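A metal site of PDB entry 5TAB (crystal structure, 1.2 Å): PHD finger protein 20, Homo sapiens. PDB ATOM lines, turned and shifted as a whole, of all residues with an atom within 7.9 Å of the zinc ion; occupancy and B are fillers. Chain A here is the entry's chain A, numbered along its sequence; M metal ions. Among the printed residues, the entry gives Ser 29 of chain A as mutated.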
ATOM      1  N   ARG A   9     -15.590  17.167  -1.520  1.00  0.00           N
ATOM      2  CA  ARG A   9     -14.583  16.864  -2.551  1.00  0.00           C
ATOM      3  C   ARG A   9     -13.297  16.506  -1.829  1.00  0.00           C
ATOM      4  O   ARG A   9     -12.480  17.368  -1.492  1.00  0.00           O
ATOM      5  CB  ARG A   9     -14.413  17.999  -3.538  1.00  0.00           C
ATOM      6  CG  ARG A   9     -13.708  17.549  -4.823  1.00  0.00           C
ATOM      7  CD  ARG A   9     -12.220  17.754  -4.752  1.00  0.00           C
ATOM      8  NE  ARG A   9     -11.788  19.127  -4.971  1.00  0.00           N
ATOM      9  CZ  ARG A   9     -11.145  19.925  -4.099  1.00  0.00           C
ATOM     10  NH1 ARG A   9     -10.960  19.546  -2.843  1.00  0.00           N
ATOM     11  NH2 ARG A   9     -10.705  21.110  -4.479  1.00  0.00           N
ATOM     12  N   GLN A  23     -13.852  22.620   5.907  1.00  0.00           N
ATOM     13  CA  GLN A  23     -14.098  23.367   4.687  1.00  0.00           C
ATOM     14  C   GLN A  23     -12.841  24.153   4.285  1.00  0.00           C
ATOM     15  O   GLN A  23     -12.284  24.926   5.084  1.00  0.00           O
ATOM     16  CB  GLN A  23     -15.261  24.343   4.890  1.00  0.00           C
ATOM     17  CG  GLN A  23     -15.699  24.982   3.596  1.00  0.00           C
ATOM     18  CD  GLN A  23     -16.880  25.902   3.740  1.00  0.00           C
ATOM     19  OE1 GLN A  23     -17.188  26.373   4.821  1.00  0.00           O
ATOM     20  NE2 GLN A  23     -17.531  26.204   2.606  1.00  0.00           N
ATOM     21  N   CYS A  24     -12.397  23.947   3.043  1.00  0.00           N
ATOM     22  CA  CYS A  24     -11.189  24.600   2.554  1.00  0.00           C
ATOM     23  C   CYS A  24     -11.413  26.089   2.388  1.00  0.00           C
ATOM     24  O   CYS A  24     -12.415  26.519   1.770  1.00  0.00           O
ATOM     25  CB  CYS A  24     -10.811  23.992   1.197  1.00  0.00           C
ATOM     26  SG  CYS A  24      -9.321  24.747   0.484  1.00  0.00           S
ATOM     27  N   GLU A  25     -10.461  26.893   2.873  1.00  0.00           N
ATOM     28  CA  GLU A  25     -10.607  28.342   2.774  1.00  0.00           C
ATOM     29  C   GLU A  25     -10.528  28.840   1.329  1.00  0.00           C
ATOM     30  O   GLU A  25     -11.030  29.911   0.995  1.00  0.00           O
ATOM     31  CB  GLU A  25      -9.527  29.054   3.609  1.00  0.00           C
ATOM     32  CG  GLU A  25      -9.751  30.548   3.700  1.00  0.00           C
ATOM     33  CD  GLU A  25      -9.125  31.175   4.890  1.00  0.00           C
ATOM     34  OE1 GLU A  25      -9.863  31.527   5.830  1.00  0.00           O
ATOM     35  OE2 GLU A  25      -7.900  31.333   4.857  1.00  0.00           O
ATOM     36  N   GLU A  26      -9.860  28.077   0.449  1.00  0.00           N
ATOM     37  CA  GLU A  26      -9.607  28.515  -0.916  1.00  0.00           C
ATOM     38  C   GLU A  26     -10.736  28.046  -1.844  1.00  0.00           C
ATOM     39  O   GLU A  26     -11.435  28.862  -2.405  1.00  0.00           O
ATOM     40  CB  GLU A  26      -8.251  28.000  -1.403  1.00  0.00           C
ATOM     41  CG  GLU A  26      -7.825  28.648  -2.642  1.00  0.00           C
ATOM     42  CD  GLU A  26      -7.573  30.142  -2.413  1.00  0.00           C
ATOM     43  OE1 GLU A  26      -7.014  30.521  -1.346  1.00  0.00           O
ATOM     44  OE2 GLU A  26      -7.973  30.932  -3.298  1.00  0.00           O
ATOM     45  N   CYS A  27     -10.979  26.744  -1.983  1.00  0.00           N
ATOM     46  CA  CYS A  27     -11.953  26.247  -2.961  1.00  0.00           C
ATOM     47  C   CYS A  27     -13.343  26.145  -2.354  1.00  0.00           C
ATOM     48  O   CYS A  27     -14.302  25.949  -3.103  1.00  0.00           O
ATOM     49  CB  CYS A  27     -11.534  24.892  -3.543  1.00  0.00           C
ATOM     50  SG  CYS A  27     -11.504  23.554  -2.297  1.00  0.00           S
ATOM     51  N   GLN A  28     -13.453  26.220  -1.029  1.00  0.00           N
ATOM     52  CA  GLN A  28     -14.750  26.232  -0.305  1.00  0.00           C
ATOM     53  C   GLN A  28     -15.460  24.877  -0.283  1.00  0.00           C
ATOM     54  O   GLN A  28     -16.567  24.792   0.255  1.00  0.00           O
ATOM     55  CB  GLN A  28     -15.680  27.368  -0.793  1.00  0.00           C
ATOM     56  CG  GLN A  28     -15.037  28.751  -0.561  1.00  0.00           C
ATOM     57  CD  GLN A  28     -15.710  29.900  -1.302  1.00  0.00           C
ATOM     58  OE1 GLN A  28     -16.382  29.722  -2.326  1.00  0.00           O
ATOM     59  NE2 GLN A  28     -15.490  31.110  -0.782  1.00  0.00           N
ATOM     60  N   SER A  29     -14.858  23.808  -0.834  1.00  0.00           N
ATOM     61  CA  SER A  29     -15.416  22.478  -0.698  1.00  0.00           C
ATOM     62  C   SER A  29     -14.925  21.862   0.628  1.00  0.00           C
ATOM     63  O   SER A  29     -14.047  22.397   1.297  1.00  0.00           O
ATOM     64  CB  SER A  29     -15.046  21.590  -1.859  1.00  0.00           C
ATOM     65  OG  SER A  29     -13.672  21.236  -1.856  1.00  0.00           O
ATOM     66  N   TRP A  30     -15.520  20.725   0.976  1.00  0.00           N
ATOM     67  CA  TRP A  30     -15.294  20.072   2.260  1.00  0.00           C
ATOM     68  C   TRP A  30     -14.564  18.751   2.079  1.00  0.00           C
ATOM     69  O   TRP A  30     -14.792  18.026   1.115  1.00  0.00           O
ATOM     70  CB  TRP A  30     -16.619  19.825   2.980  1.00  0.00           C
ATOM     71  CG  TRP A  30     -17.370  21.077   3.374  1.00  0.00           C
ATOM     72  CD1 TRP A  30     -18.045  21.929   2.540  1.00  0.00           C
ATOM     73  CD2 TRP A  30     -17.569  21.576   4.702  1.00  0.00           C
ATOM     74  NE1 TRP A  30     -18.645  22.930   3.265  1.00  0.00           N
ATOM     75  CE2 TRP A  30     -18.367  22.732   4.604  1.00  0.00           C
ATOM     76  CE3 TRP A  30     -17.153  21.149   5.973  1.00  0.00           C
ATOM     77  CZ2 TRP A  30     -18.764  23.460   5.720  1.00  0.00           C
ATOM     78  CZ3 TRP A  30     -17.538  21.882   7.084  1.00  0.00           C
ATOM     79  CH2 TRP A  30     -18.364  23.017   6.957  1.00  0.00           C
ATOM     80  N   GLN A  31     -13.737  18.425   3.061  1.00  0.00           N
ATOM     81  CA  GLN A  31     -12.995  17.174   3.110  1.00  0.00           C
ATOM     82  C   GLN A  31     -13.240  16.492   4.454  1.00  0.00           C
ATOM     83  O   GLN A  31     -13.636  17.138   5.456  1.00  0.00           O
ATOM     84  CB  GLN A  31     -11.493  17.437   2.960  1.00  0.00           C
ATOM     85  CG  GLN A  31     -11.116  18.012   1.612  1.00  0.00           C
ATOM     86  CD  GLN A  31     -11.474  19.476   1.455  1.00  0.00           C
ATOM     87  OE1 GLN A  31     -11.152  20.321   2.310  1.00  0.00           O
ATOM     88  NE2 GLN A  31     -12.157  19.827   0.333  1.00  0.00           N
ATOM     89  N   TYR A  47      -7.336  26.650   7.196  1.00  0.00           N
ATOM     90  CA  TYR A  47      -7.111  25.370   6.558  1.00  0.00           C
ATOM     91  C   TYR A  47      -7.328  25.425   5.052  1.00  0.00           C
ATOM     92  O   TYR A  47      -8.312  25.946   4.561  1.00  0.00           O
ATOM     93  CB  TYR A  47      -8.058  24.336   7.202  1.00  0.00           C
ATOM     94  CG  TYR A  47      -8.321  23.161   6.325  1.00  0.00           C
ATOM     95  CD1 TYR A  47      -7.348  22.167   6.159  1.00  0.00           C
ATOM     96  CD2 TYR A  47      -9.529  23.047   5.645  1.00  0.00           C
ATOM     97  CE1 TYR A  47      -7.567  21.105   5.299  1.00  0.00           C
ATOM     98  CE2 TYR A  47      -9.757  21.995   4.775  1.00  0.00           C
ATOM     99  CZ  TYR A  47      -8.774  21.036   4.589  1.00  0.00           C
ATOM    100  OH  TYR A  47      -8.969  19.969   3.743  1.00  0.00           O
ATOM    101  N   THR A  48      -6.396  24.790   4.359  1.00  0.00           N
ATOM    102  CA  THR A  48      -6.396  24.640   2.915  1.00  0.00           C
ATOM    103  C   THR A  48      -6.212  23.171   2.542  1.00  0.00           C
ATOM    104  O   THR A  48      -5.365  22.504   3.109  1.00  0.00           O
ATOM    105  CB  THR A  48      -5.234  25.462   2.345  1.00  0.00           C
ATOM    106  OG1 THR A  48      -5.337  26.796   2.877  1.00  0.00           O
ATOM    107  CG2 THR A  48      -5.244  25.474   0.841  1.00  0.00           C
ATOM    108  N   CYS A  49      -7.039  22.700   1.606  1.00  0.00           N
ATOM    109  CA  CYS A  49      -7.111  21.278   1.291  1.00  0.00           C
ATOM    110  C   CYS A  49      -5.954  20.755   0.444  1.00  0.00           C
ATOM    111  O   CYS A  49      -5.070  21.511   0.005  1.00  0.00           O
ATOM    112  CB  CYS A  49      -8.441  20.927   0.602  1.00  0.00           C
ATOM    113  SG  CYS A  49      -8.495  21.363  -1.161  1.00  0.00           S
ATOM    114  N   TYR A  50      -5.963  19.449   0.215  1.00  0.00           N
ATOM    115  CA  TYR A  50      -4.917  18.738  -0.515  1.00  0.00           C
ATOM    116  C   TYR A  50      -4.721  19.273  -1.922  1.00  0.00           C
ATOM    117  O   TYR A  50      -3.607  19.222  -2.457  1.00  0.00           O
ATOM    118  CB  TYR A  50      -5.239  17.244  -0.579  1.00  0.00           C
ATOM    119  CG  TYR A  50      -6.445  16.869  -1.446  1.00  0.00           C
ATOM    120  CD1 TYR A  50      -7.752  17.094  -1.006  1.00  0.00           C
ATOM    121  CD2 TYR A  50      -6.279  16.201  -2.643  1.00  0.00           C
ATOM    122  CE1 TYR A  50      -8.851  16.716  -1.758  1.00  0.00           C
ATOM    123  CE2 TYR A  50      -7.364  15.788  -3.415  1.00  0.00           C
ATOM    124  CZ  TYR A  50      -8.657  16.066  -2.969  1.00  0.00           C
ATOM    125  OH  TYR A  50      -9.756  15.681  -3.709  1.00  0.00           O
ATOM    126  N   VAL A  51      -5.803  19.753  -2.544  1.00  0.00           N
ATOM    127  CA  VAL A  51      -5.700  20.274  -3.894  1.00  0.00           C
ATOM    128  C   VAL A  51      -5.070  21.649  -3.914  1.00  0.00           C
ATOM    129  O   VAL A  51      -4.213  21.919  -4.788  1.00  0.00           O
ATOM    130  CB  VAL A  51      -7.109  20.343  -4.583  1.00  0.00           C
ATOM    131  CG1 VAL A  51      -7.042  21.110  -5.936  1.00  0.00           C
ATOM    132  CG2 VAL A  51      -7.638  18.948  -4.788  1.00  0.00           C
ATOM    133  N   CYS A  52      -5.483  22.492  -2.976  1.00  0.00           N
ATOM    134  CA  CYS A  52      -5.210  23.916  -2.979  1.00  0.00           C
ATOM    135  C   CYS A  52      -3.907  24.286  -2.295  1.00  0.00           C
ATOM    136  O   CYS A  52      -3.385  25.350  -2.540  1.00  0.00           O
ATOM    137  CB  CYS A  52      -6.366  24.678  -2.286  1.00  0.00           C
ATOM    138  SG  CYS A  52      -7.958  24.516  -3.145  1.00  0.00           S
ATOM    139  N   GLN A  53      -3.410  23.430  -1.399  1.00  0.00           N
ATOM    140  CA  GLN A  53      -2.271  23.804  -0.616  1.00  0.00           C
ATOM    141  C   GLN A  53      -0.992  23.863  -1.488  1.00  0.00           C
ATOM    142  O   GLN A  53      -0.028  24.509  -1.031  1.00  0.00           O
ATOM    143  CB  GLN A  53      -2.132  22.889   0.619  1.00  0.00           C
ATOM    144  CG  GLN A  53      -1.745  21.484   0.261  1.00  0.00           C
ATOM    145  CD  GLN A  53      -1.552  20.559   1.458  1.00  0.00           C
ATOM    146  OE1 GLN A  53      -2.015  19.453   1.432  1.00  0.00           O
ATOM    147  NE2 GLN A  53      -0.825  20.984   2.480  1.00  0.00           N
HETATM  148 ZN    ZN M   1      -9.289  23.516  -1.516  1.00  0.00          ZN
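The side-chain sulfur of Cys 49 lies close to the guanidinium group of Arg 9 (3.5 Å).
The backbone NH of Val 51 lies close to the side-chain sulfur of Cys 49 (3.4 Å).
The side-chain sulfur of Cys 27 sits close to the guanidinium group of Arg 9.
The side-chain sulfur of Cys 27 lies close to the side-chain hydroxyl of Ser 29, 3.2 Å away.
The side-chain sulfur (SG) of Cys 24 lies close to the backbone NH (N) of Glu 26 (3.4 Å).
N of Cys 24 sits at hydrogen-bond distance from O of Ser 29, at 2.9 Å.
Within 4 Å of the zinc ion: Cys 24, Cys 27, Cys 49 and Cys 52.
The nearest printed residue that does not touch the zinc ion is Arg 9 (4.1 Å).
The zinc ion is bound by SG of Cys 49 (2.3 Å).
The zinc ion is bound by SG of Cys 52 (2.3 Å).
The side-chain sulfur (SG) of Cys 27 is bound to the zinc ion (2.3 Å).
SG of Cys 24 binds the zinc ion (2.3 Å).
The zinc ion has four donor atoms within binding distance.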
